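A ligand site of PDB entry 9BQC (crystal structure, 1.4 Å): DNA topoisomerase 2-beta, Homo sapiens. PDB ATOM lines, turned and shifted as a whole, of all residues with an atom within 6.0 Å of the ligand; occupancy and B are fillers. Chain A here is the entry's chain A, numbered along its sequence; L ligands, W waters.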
ATOM      1  N   LEU A  32       4.817   6.902 -12.797  1.00  0.00           N
ATOM      2  CA  LEU A  32       3.901   7.486 -13.769  1.00  0.00           C
ATOM      3  C   LEU A  32       2.547   6.847 -13.492  1.00  0.00           C
ATOM      4  O   LEU A  32       2.482   5.645 -13.206  1.00  0.00           O
ATOM      5  CB  LEU A  32       4.341   7.127 -15.199  1.00  0.00           C
ATOM      6  CG  LEU A  32       3.440   7.538 -16.369  1.00  0.00           C
ATOM      7  CD1 LEU A  32       3.235   9.044 -16.364  1.00  0.00           C
ATOM      8  CD2 LEU A  32       4.032   7.063 -17.703  1.00  0.00           C
ATOM      9  N   GLN A  34      -0.984   6.232 -15.556  1.00  0.00           N
ATOM     10  CA  GLN A  34      -1.483   6.271 -16.920  1.00  0.00           C
ATOM     11  C   GLN A  34      -2.682   5.335 -17.034  1.00  0.00           C
ATOM     12  O   GLN A  34      -2.695   4.255 -16.431  1.00  0.00           O
ATOM     13  CB  GLN A  34      -0.370   5.845 -17.907  1.00  0.00           C
ATOM     14  CG  GLN A  34      -0.676   6.143 -19.365  1.00  0.00           C
ATOM     15  CD  GLN A  34       0.547   6.054 -20.258  1.00  0.00           C
ATOM     16  OE1 GLN A  34       1.640   5.690 -19.825  1.00  0.00           O
ATOM     17  NE2 GLN A  34       0.359   6.384 -21.531  1.00  0.00           N
ATOM     18  N   PHE A  35      -3.695   5.761 -17.773  1.00  0.00           N
ATOM     19  CA  PHE A  35      -4.835   4.898 -18.083  1.00  0.00           C
ATOM     20  C   PHE A  35      -4.417   3.987 -19.215  1.00  0.00           C
ATOM     21  O   PHE A  35      -4.080   4.474 -20.302  1.00  0.00           O
ATOM     22  CB  PHE A  35      -6.013   5.769 -18.490  1.00  0.00           C
ATOM     23  CG  PHE A  35      -7.312   5.030 -18.630  1.00  0.00           C
ATOM     24  CD1 PHE A  35      -8.021   4.634 -17.516  1.00  0.00           C
ATOM     25  CD2 PHE A  35      -7.827   4.737 -19.878  1.00  0.00           C
ATOM     26  CE1 PHE A  35      -9.216   3.952 -17.634  1.00  0.00           C
ATOM     27  CE2 PHE A  35      -9.029   4.074 -20.015  1.00  0.00           C
ATOM     28  CZ  PHE A  35      -9.721   3.665 -18.889  1.00  0.00           C
ATOM     29  N   MET A  36      -4.393   2.688 -18.985  1.00  0.00           N
ATOM     30  CA  MET A  36      -3.858   1.772 -19.976  1.00  0.00           C
ATOM     31  C   MET A  36      -4.375   0.367 -19.695  1.00  0.00           C
ATOM     32  O   MET A  36      -5.062   0.128 -18.704  1.00  0.00           O
ATOM     33  CB  MET A  36      -2.332   1.773 -19.973  1.00  0.00           C
ATOM     34  CG  MET A  36      -1.775   1.376 -18.625  1.00  0.00           C
ATOM     35  SD  MET A  36      -0.020   1.566 -18.462  1.00  0.00           S
ATOM     36  CE  MET A  36       0.403   0.228 -19.504  1.00  0.00           C
ATOM     37  N   TRP A  37      -4.002  -0.570 -20.563  1.00  0.00           N
ATOM     38  CA  TRP A  37      -4.425  -1.962 -20.458  1.00  0.00           C
ATOM     39  C   TRP A  37      -3.404  -2.778 -19.696  1.00  0.00           C
ATOM     40  O   TRP A  37      -2.200  -2.706 -19.974  1.00  0.00           O
ATOM     41  CB  TRP A  37      -4.623  -2.551 -21.856  1.00  0.00           C
ATOM     42  CG  TRP A  37      -5.679  -1.867 -22.668  1.00  0.00           C
ATOM     43  CD1 TRP A  37      -5.499  -0.835 -23.532  1.00  0.00           C
ATOM     44  CD2 TRP A  37      -7.071  -2.187 -22.711  1.00  0.00           C
ATOM     45  NE1 TRP A  37      -6.697  -0.469 -24.095  1.00  0.00           N
ATOM     46  CE2 TRP A  37      -7.682  -1.294 -23.611  1.00  0.00           C
ATOM     47  CE3 TRP A  37      -7.868  -3.150 -22.066  1.00  0.00           C
ATOM     48  CZ2 TRP A  37      -9.043  -1.320 -23.884  1.00  0.00           C
ATOM     49  CZ3 TRP A  37      -9.212  -3.165 -22.335  1.00  0.00           C
ATOM     50  CH2 TRP A  37      -9.793  -2.263 -23.239  1.00  0.00           C
ATOM     51  N   VAL A  38      -3.867  -3.565 -18.732  1.00  0.00           N
ATOM     52  CA  VAL A  38      -3.011  -4.527 -18.053  1.00  0.00           C
ATOM     53  C   VAL A  38      -3.796  -5.822 -17.878  1.00  0.00           C
ATOM     54  O   VAL A  38      -5.008  -5.881 -18.119  1.00  0.00           O
ATOM     55  CB  VAL A  38      -2.495  -4.016 -16.701  1.00  0.00           C
ATOM     56  CG1 VAL A  38      -1.576  -2.788 -16.891  1.00  0.00           C
ATOM     57  CG2 VAL A  38      -3.646  -3.675 -15.781  1.00  0.00           C
ATOM     58  N   CYS A  47      -8.770  -2.093 -18.769  1.00  0.00           N
ATOM     59  CA  CYS A  47      -8.185  -0.773 -18.894  1.00  0.00           C
ATOM     60  C   CYS A  47      -8.492  -0.004 -17.625  1.00  0.00           C
ATOM     61  O   CYS A  47      -9.664   0.066 -17.204  1.00  0.00           O
ATOM     62  CB  CYS A  47      -8.726  -0.053 -20.126  1.00  0.00           C
ATOM     63  SG  CYS A  47      -7.643   1.231 -20.761  1.00  0.00           S
ATOM     64  N   PHE A  52       3.185   2.944 -12.279  1.00  0.00           N
ATOM     65  CA  PHE A  52       4.353   2.094 -12.514  1.00  0.00           C
ATOM     66  C   PHE A  52       5.520   2.980 -12.901  1.00  0.00           C
ATOM     67  O   PHE A  52       5.346   4.143 -13.251  1.00  0.00           O
ATOM     68  CB  PHE A  52       4.083   1.066 -13.611  1.00  0.00           C
ATOM     69  CG  PHE A  52       3.979   1.653 -14.976  1.00  0.00           C
ATOM     70  CD1 PHE A  52       2.851   2.367 -15.360  1.00  0.00           C
ATOM     71  CD2 PHE A  52       5.022   1.505 -15.875  1.00  0.00           C
ATOM     72  CE1 PHE A  52       2.770   2.923 -16.632  1.00  0.00           C
ATOM     73  CE2 PHE A  52       4.946   2.053 -17.147  1.00  0.00           C
ATOM     74  CZ  PHE A  52       3.824   2.758 -17.531  1.00  0.00           C
ATOM     75  N   PRO A  54       8.300   3.540 -15.636  1.00  0.00           N
ATOM     76  CA  PRO A  54       8.592   3.107 -17.007  1.00  0.00           C
ATOM     77  C   PRO A  54       9.906   2.367 -17.186  1.00  0.00           C
ATOM     78  O   PRO A  54       9.946   1.391 -17.930  1.00  0.00           O
ATOM     79  CB  PRO A  54       8.546   4.435 -17.798  1.00  0.00           C
ATOM     80  CG  PRO A  54       7.534   5.261 -17.019  1.00  0.00           C
ATOM     81  CD  PRO A  54       7.813   4.933 -15.568  1.00  0.00           C
ATOM     82  N   TYR A  57       9.510  -1.396 -16.337  1.00  0.00           N
ATOM     83  CA  TYR A  57       8.843  -2.016 -17.471  1.00  0.00           C
ATOM     84  C   TYR A  57       9.822  -2.257 -18.614  1.00  0.00           C
ATOM     85  O   TYR A  57       9.872  -3.344 -19.194  1.00  0.00           O
ATOM     86  CB  TYR A  57       7.637  -1.152 -17.893  1.00  0.00           C
ATOM     87  CG  TYR A  57       7.220  -1.238 -19.358  1.00  0.00           C
ATOM     88  CD1 TYR A  57       6.620  -2.383 -19.870  1.00  0.00           C
ATOM     89  CD2 TYR A  57       7.387  -0.155 -20.209  1.00  0.00           C
ATOM     90  CE1 TYR A  57       6.242  -2.443 -21.214  1.00  0.00           C
ATOM     91  CE2 TYR A  57       7.021  -0.231 -21.552  1.00  0.00           C
ATOM     92  CZ  TYR A  57       6.442  -1.361 -22.039  1.00  0.00           C
ATOM     93  OH  TYR A  57       6.067  -1.407 -23.381  1.00  0.00           O
ATOM     94  N   LEU A 213       1.281  -5.288 -15.764  1.00  0.00           N
ATOM     95  CA  LEU A 213       1.795  -4.782 -17.033  1.00  0.00           C
ATOM     96  C   LEU A 213       2.752  -5.776 -17.675  1.00  0.00           C
ATOM     97  O   LEU A 213       2.666  -6.049 -18.879  1.00  0.00           O
ATOM     98  CB  LEU A 213       2.474  -3.433 -16.803  1.00  0.00           C
ATOM     99  CG  LEU A 213       3.188  -2.771 -17.961  1.00  0.00           C
ATOM    100  CD1 LEU A 213       2.323  -2.683 -19.209  1.00  0.00           C
ATOM    101  CD2 LEU A 213       3.657  -1.378 -17.538  1.00  0.00           C
ATOM    102  N   ARG A 216       0.788  -8.560 -19.051  1.00  0.00           N
ATOM    103  CA  ARG A 216       0.137  -8.236 -20.311  1.00  0.00           C
ATOM    104  C   ARG A 216       1.114  -8.299 -21.477  1.00  0.00           C
ATOM    105  O   ARG A 216       0.742  -8.711 -22.580  1.00  0.00           O
ATOM    106  CB  ARG A 216      -0.550  -6.856 -20.288  1.00  0.00           C
ATOM    107  CG  ARG A 216      -1.664  -6.764 -21.373  1.00  0.00           C
ATOM    108  CD  ARG A 216      -1.752  -5.367 -22.022  1.00  0.00           C
ATOM    109  NE  ARG A 216      -0.529  -5.071 -22.754  1.00  0.00           N
ATOM    110  CZ  ARG A 216       0.335  -4.102 -22.449  1.00  0.00           C
ATOM    111  NH1 ARG A 216       0.067  -3.167 -21.554  1.00  0.00           N
ATOM    112  NH2 ARG A 216       1.512  -4.063 -23.093  1.00  0.00           N
ATOM    113  N   ARG A 217       2.373  -7.873 -21.273  1.00  0.00           N
ATOM    114  CA  ARG A 217       3.336  -7.980 -22.364  1.00  0.00           C
ATOM    115  C   ARG A 217       3.528  -9.427 -22.794  1.00  0.00           C
ATOM    116  O   ARG A 217       3.778  -9.682 -23.970  1.00  0.00           O
ATOM    117  CB  ARG A 217       4.693  -7.367 -21.961  1.00  0.00           C
ATOM    118  CG  ARG A 217       4.757  -5.851 -21.981  1.00  0.00           C
ATOM    119  CD  ARG A 217       4.686  -5.242 -23.389  1.00  0.00           C
ATOM    120  NE  ARG A 217       5.836  -5.535 -24.234  1.00  0.00           N
ATOM    121  CZ  ARG A 217       5.762  -6.039 -25.459  1.00  0.00           C
ATOM    122  NH1 ARG A 217       4.611  -6.350 -26.031  1.00  0.00           N
ATOM    123  NH2 ARG A 217       6.886  -6.240 -26.135  1.00  0.00           N
ATOM    124  N   ASP A 220       0.718 -10.000 -25.079  1.00  0.00           N
ATOM    125  CA  ASP A 220       1.024  -9.320 -26.324  1.00  0.00           C
ATOM    126  C   ASP A 220       1.876 -10.217 -27.208  1.00  0.00           C
ATOM    127  O   ASP A 220       1.636 -10.352 -28.404  1.00  0.00           O
ATOM    128  CB  ASP A 220       1.868  -8.065 -26.065  1.00  0.00           C
ATOM    129  CG  ASP A 220       1.172  -6.934 -25.304  1.00  0.00           C
ATOM    130  OD1 ASP A 220      -0.031  -7.079 -25.033  1.00  0.00           O
ATOM    131  OD2 ASP A 220       1.853  -5.931 -24.997  1.00  0.00           O
ATOM    132  N   TYR A 245      -5.872 -12.542 -29.810  1.00  0.00           N
ATOM    133  CA  TYR A 245      -5.375 -11.510 -28.909  1.00  0.00           C
ATOM    134  C   TYR A 245      -6.299 -10.298 -28.912  1.00  0.00           C
ATOM    135  O   TYR A 245      -6.685  -9.775 -27.865  1.00  0.00           O
ATOM    136  CB  TYR A 245      -3.947 -11.135 -29.333  1.00  0.00           C
ATOM    137  CG  TYR A 245      -3.412  -9.935 -28.592  1.00  0.00           C
ATOM    138  CD1 TYR A 245      -2.878 -10.049 -27.321  1.00  0.00           C
ATOM    139  CD2 TYR A 245      -3.448  -8.659 -29.173  1.00  0.00           C
ATOM    140  CE1 TYR A 245      -2.399  -8.934 -26.628  1.00  0.00           C
ATOM    141  CE2 TYR A 245      -2.975  -7.549 -28.492  1.00  0.00           C
ATOM    142  CZ  TYR A 245      -2.445  -7.689 -27.234  1.00  0.00           C
ATOM    143  OH  TYR A 245      -1.985  -6.563 -26.595  1.00  0.00           O
ATOM    144  N   TYR A 249      -9.652  -7.652 -26.011  1.00  0.00           N
ATOM    145  CA  TYR A 249     -10.084  -6.270 -25.884  1.00  0.00           C
ATOM    146  C   TYR A 249     -11.524  -6.051 -26.308  1.00  0.00           C
ATOM    147  O   TYR A 249     -12.212  -5.252 -25.681  1.00  0.00           O
ATOM    148  CB  TYR A 249      -9.203  -5.386 -26.767  1.00  0.00           C
ATOM    149  CG  TYR A 249      -7.755  -5.325 -26.343  1.00  0.00           C
ATOM    150  CD1 TYR A 249      -6.830  -6.265 -26.791  1.00  0.00           C
ATOM    151  CD2 TYR A 249      -7.316  -4.331 -25.496  1.00  0.00           C
ATOM    152  CE1 TYR A 249      -5.524  -6.202 -26.391  1.00  0.00           C
ATOM    153  CE2 TYR A 249      -5.996  -4.247 -25.112  1.00  0.00           C
ATOM    154  CZ  TYR A 249      -5.117  -5.193 -25.558  1.00  0.00           C
ATOM    155  OH  TYR A 249      -3.812  -5.106 -25.166  1.00  0.00           O
ATOM    156  N   GLN A 284      -7.902   5.529 -30.971  1.00  0.00           N
ATOM    157  CA  GLN A 284      -7.184   4.549 -30.174  1.00  0.00           C
ATOM    158  C   GLN A 284      -6.415   3.645 -31.103  1.00  0.00           C
ATOM    159  O   GLN A 284      -6.964   3.164 -32.090  1.00  0.00           O
ATOM    160  CB  GLN A 284      -8.152   3.667 -29.396  1.00  0.00           C
ATOM    161  CG  GLN A 284      -9.040   4.325 -28.410  1.00  0.00           C
ATOM    162  CD  GLN A 284      -9.885   3.284 -27.710  1.00  0.00           C
ATOM    163  OE1 GLN A 284      -9.369   2.483 -26.919  1.00  0.00           O
ATOM    164  NE2 GLN A 284     -11.186   3.261 -28.034  1.00  0.00           N
ATOM    165  N   GLN A 285      -5.156   3.377 -30.765  1.00  0.00           N
ATOM    166  CA  GLN A 285      -4.384   2.405 -31.517  1.00  0.00           C
ATOM    167  C   GLN A 285      -3.665   1.476 -30.552  1.00  0.00           C
ATOM    168  O   GLN A 285      -3.165   1.901 -29.508  1.00  0.00           O
ATOM    169  CB  GLN A 285      -3.373   3.062 -32.463  1.00  0.00           C
ATOM    170  CG  GLN A 285      -2.260   3.864 -31.766  1.00  0.00           C
ATOM    171  CD  GLN A 285      -1.058   3.032 -31.362  1.00  0.00           C
ATOM    172  OE1 GLN A 285      -0.915   1.876 -31.780  1.00  0.00           O
ATOM    173  NE2 GLN A 285      -0.169   3.616 -30.551  1.00  0.00           N
ATOM    174  N   ILE A 286      -3.661   0.193 -30.905  1.00  0.00           N
ATOM    175  CA  ILE A 286      -2.825  -0.831 -30.276  1.00  0.00           C
ATOM    176  C   ILE A 286      -1.999  -1.435 -31.410  1.00  0.00           C
ATOM    177  O   ILE A 286      -2.553  -1.944 -32.401  1.00  0.00           O
ATOM    178  CB  ILE A 286      -3.687  -1.871 -29.558  1.00  0.00           C
ATOM    179  CG1 ILE A 286      -4.313  -1.241 -28.306  1.00  0.00           C
ATOM    180  CG2 ILE A 286      -2.896  -3.095 -29.212  1.00  0.00           C
ATOM    181  CD1 ILE A 286      -5.215  -2.151 -27.521  1.00  0.00           C
ATOM    182  N   SER A 287      -0.682  -1.344 -31.291  1.00  0.00           N
ATOM    183  CA  SER A 287       0.169  -1.729 -32.419  1.00  0.00           C
ATOM    184  C   SER A 287       1.485  -2.317 -31.940  1.00  0.00           C
ATOM    185  O   SER A 287       2.004  -1.963 -30.880  1.00  0.00           O
ATOM    186  CB  SER A 287       0.439  -0.530 -33.353  1.00  0.00           C
ATOM    187  OG  SER A 287       1.109   0.531 -32.695  1.00  0.00           O
ATOM    188  N   PHE A 288       2.037  -3.183 -32.780  1.00  0.00           N
ATOM    189  CA  PHE A 288       3.303  -3.867 -32.544  1.00  0.00           C
ATOM    190  C   PHE A 288       4.107  -3.830 -33.831  1.00  0.00           C
ATOM    191  O   PHE A 288       3.570  -4.052 -34.923  1.00  0.00           O
ATOM    192  CB  PHE A 288       3.082  -5.314 -32.106  1.00  0.00           C
ATOM    193  CG  PHE A 288       2.205  -5.426 -30.920  1.00  0.00           C
ATOM    194  CD1 PHE A 288       2.721  -5.311 -29.649  1.00  0.00           C
ATOM    195  CD2 PHE A 288       0.841  -5.525 -31.078  1.00  0.00           C
ATOM    196  CE1 PHE A 288       1.883  -5.361 -28.542  1.00  0.00           C
ATOM    197  CE2 PHE A 288       0.006  -5.549 -29.958  1.00  0.00           C
ATOM    198  CZ  PHE A 288       0.526  -5.468 -28.710  1.00  0.00           C
ATOM    199  N   ALA A 293       5.857  -3.205 -28.489  1.00  0.00           N
ATOM    200  CA  ALA A 293       4.631  -2.407 -28.331  1.00  0.00           C
ATOM    201  C   ALA A 293       4.939  -0.949 -28.651  1.00  0.00           C
ATOM    202  O   ALA A 293       5.644  -0.272 -27.893  1.00  0.00           O
ATOM    203  CB  ALA A 293       4.075  -2.531 -26.918  1.00  0.00           C
ATOM    204  N   THR A 294       4.450  -0.469 -29.796  1.00  0.00           N
ATOM    205  CA  THR A 294       4.679   0.912 -30.240  1.00  0.00           C
ATOM    206  C   THR A 294       3.614   1.832 -29.655  1.00  0.00           C
ATOM    207  O   THR A 294       2.630   2.219 -30.301  1.00  0.00           O
ATOM    208  CB  THR A 294       4.809   0.994 -31.749  1.00  0.00           C
ATOM    209  OG1 THR A 294       3.765   0.250 -32.387  1.00  0.00           O
ATOM    210  CG2 THR A 294       6.129   0.398 -32.198  1.00  0.00           C
ATOM    211  N   THR A 295       3.812   2.145 -28.367  1.00  0.00           N
ATOM    212  CA  THR A 295       2.798   2.790 -27.535  1.00  0.00           C
ATOM    213  C   THR A 295       2.604   4.264 -27.847  1.00  0.00           C
ATOM    214  O   THR A 295       1.636   4.853 -27.370  1.00  0.00           O
ATOM    215  CB  THR A 295       3.125   2.542 -26.048  1.00  0.00           C
ATOM    216  OG1 THR A 295       4.502   2.843 -25.785  1.00  0.00           O
ATOM    217  CG2 THR A 295       2.910   1.086 -25.711  1.00  0.00           C
ATOM    218  N   LYS A 296       3.466   4.861 -28.671  1.00  0.00           N
ATOM    219  CA  LYS A 296       3.219   6.189 -29.231  1.00  0.00           C
ATOM    220  C   LYS A 296       2.950   6.128 -30.720  1.00  0.00           C
ATOM    221  O   LYS A 296       2.863   7.178 -31.383  1.00  0.00           O
ATOM    222  CB  LYS A 296       4.405   7.096 -28.929  1.00  0.00           C
ATOM    223  CG  LYS A 296       4.491   7.455 -27.452  1.00  0.00           C
ATOM    224  CD  LYS A 296       5.659   8.397 -27.170  1.00  0.00           C
ATOM    225  CE  LYS A 296       5.765   8.723 -25.682  1.00  0.00           C
ATOM    226  NZ  LYS A 296       4.504   9.334 -25.161  1.00  0.00           N
ATOM    227  N   GLY A 297       2.814   4.942 -31.270  1.00  0.00           N
ATOM    228  CA  GLY A 297       2.418   4.774 -32.648  1.00  0.00           C
ATOM    229  C   GLY A 297       3.590   4.855 -33.593  1.00  0.00           C
ATOM    230  O   GLY A 297       4.669   4.311 -33.324  1.00  0.00           O
ATOM    231  N   GLU A 354       9.031   3.550 -28.526  1.00  0.00           N
ATOM    232  CA  GLU A 354       7.597   3.779 -28.480  1.00  0.00           C
ATOM    233  C   GLU A 354       7.026   4.298 -29.798  1.00  0.00           C
ATOM    234  O   GLU A 354       5.819   4.146 -30.058  1.00  0.00           O
ATOM    235  CB  GLU A 354       7.238   4.800 -27.388  1.00  0.00           C
ATOM    236  CG  GLU A 354       7.423   4.326 -25.958  1.00  0.00           C
ATOM    237  CD  GLU A 354       6.620   5.136 -24.931  1.00  0.00           C
ATOM    238  OE1 GLU A 354       5.354   5.128 -24.932  1.00  0.00           O
ATOM    239  OE2 GLU A 354       7.281   5.821 -24.109  1.00  0.00           O
HETATM  240  C1  LIG L   1       0.813   3.328 -22.751  1.00  0.00           C
HETATM  241  C2  LIG L   1       1.437   2.088 -22.638  1.00  0.00           C
HETATM  242  C3  LIG L   1      -0.529   3.468 -23.157  1.00  0.00           C
HETATM  243  C4  LIG L   1       2.773   1.896 -22.218  1.00  0.00           C
HETATM  244  C5  LIG L   1       0.658   0.970 -22.984  1.00  0.00           C
HETATM  245  C6  LIG L   1      -1.275   2.325 -23.469  1.00  0.00           C
HETATM  246  C7  LIG L   1       3.288   0.607 -22.128  1.00  0.00           C
HETATM  247  C8  LIG L   1       3.603   3.154 -21.859  1.00  0.00           C
HETATM  248  C9  LIG L   1      -0.659   1.115 -23.406  1.00  0.00           C
HETATM  249  C10 LIG L   1       2.469  -0.465 -22.487  1.00  0.00           C
HETATM  250  C11 LIG L   1       5.004   2.791 -21.282  1.00  0.00           C
HETATM  251  C12 LIG L   1      -1.390  -0.196 -23.621  1.00  0.00           C
HETATM  252  C13 LIG L   1      -3.302   3.501 -23.723  1.00  0.00           C
HETATM  253  C14 LIG L   1       5.726   4.098 -20.917  1.00  0.00           C
HETATM  254  C15 LIG L   1      -4.781   3.169 -23.986  1.00  0.00           C
HETATM  255  C16 LIG L   1      -1.966  -2.291 -24.836  1.00  0.00           C
HETATM  256  C17 LIG L   1      -0.671  -0.526 -26.009  1.00  0.00           C
HETATM  257  C18 LIG L   1      -1.086  -3.277 -25.745  1.00  0.00           C
HETATM  258  C19 LIG L   1      -0.999   0.738 -26.508  1.00  0.00           C
HETATM  259  C20 LIG L   1       0.101  -1.354 -26.696  1.00  0.00           C
HETATM  260  C21 LIG L   1       0.331  -2.706 -26.100  1.00  0.00           C
HETATM  261  C22 LIG L   1      -0.456   1.143 -27.720  1.00  0.00           C
HETATM  262  C23 LIG L   1       0.654  -0.978 -27.920  1.00  0.00           C
HETATM  263  C24 LIG L   1       0.371   0.292 -28.421  1.00  0.00           C
HETATM  264  N1  LIG L   1      -1.317  -0.952 -24.816  1.00  0.00           N
HETATM  265  O1  LIG L   1       1.217  -0.265 -22.923  1.00  0.00           O
HETATM  266  O2  LIG L   1      -2.596   2.288 -23.879  1.00  0.00           O
HETATM  267  O3  LIG L   1       2.852  -1.590 -22.454  1.00  0.00           O
HETATM  268  O4  LIG L   1      -2.018  -0.649 -22.692  1.00  0.00           O
HETATM  269  O5  LIG L   1      -4.861   2.624 -25.277  1.00  0.00           O
HETATM  270  O   HOH W   1      -3.072   3.436 -27.268  1.00  0.00           O
HETATM  271  O   HOH W   2      -7.125   1.394 -26.324  1.00  0.00           O
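An oxygen (O3) of the ligand sits at hydrogen-bond distance from the guanidinium group of Arg 216, 2.9 Å away. The backbone NH (N) of Trp 37 is in hydrogen-bond range of an oxygen (O4) of the ligand (2.9 Å). An oxygen (O3) of the ligand lies within hydrogen-bond range of the side-chain hydroxyl of Tyr 57 (3.4 Å).
Gln 34 touches the ligand (NE2 to C1, 3.3 Å). O of Phe 35 touches C13 of the ligand (3.6 Å). Met 36 touches the ligand. Phe 52 touches the ligand (CZ to C11, 3.9 Å). Leu 213 touches the ligand. OD2 of Asp 220 touches C21 of the ligand, at 3.7 Å. Tyr 245 touches the ligand (OH to C18, 3.5 Å). OH of Tyr 249 touches C18 of the ligand (3.3 Å). Gln 285 touches the ligand (O to C22, 3.3 Å). CA of Ile 286 touches C24 of the ligand, at 3.9 Å. O of Ser 287 touches C23 of the ligand, at 3.4 Å. Phe 288 touches the ligand (CZ to C21, 3.8 Å). Ala 293 touches the ligand. Thr 294 touches the ligand. CG2 of Thr 295 touches O1 of the ligand (3.5 Å). OE2 of Glu 354 touches C14 of the ligand (3.9 Å). Hydrophobic or aromatic side chains within 4 Å of the ligand: Met 36, Trp 37, Phe 52, Tyr 57, Leu 213, Ile 286, Phe 288 and Ala 293.
Water W2 lies within hydrogen-bond range of the side-chain amide oxygen (OE1) of Gln 284 (2.6 Å), an oxygen (O5) of the ligand (2.8 Å) and the indole nitrogen (NE1) of Trp 37 (2.9 Å). Water W1 bridges the backbone carbonyl oxygen of Gln 285 (2.7 Å) and an oxygen (O5) of the ligand (2.8 Å).
NH1 of Arg 216 is in hydrogen-bond range of O of Trp 37, at 2.8 Å. The guanidinium group (NH2) of Arg 216 is in salt-bridge range of the side-chain carboxylate (OD2) of Asp 220. NE2 of Gln 285 is in hydrogen-bond range of O of Thr 294 (3.1 Å). The side-chain hydroxyl (OH) of Tyr 249 sits at hydrogen-bond distance from the side-chain hydroxyl (OH) of Tyr 245 (2.7 Å). The side-chain hydroxyl (OH) of Tyr 245 lies within hydrogen-bond range of the side-chain carboxylate (OD1) of Asp 220. OD2 of Asp 220 is in salt-bridge range of NH1 of Arg 217. The backbone carbonyl oxygen of Glu 354 is in hydrogen-bond range of the backbone NH of Lys 296 (2.8 Å). O of Glu 354 sits at hydrogen-bond distance from N of Gly 297.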
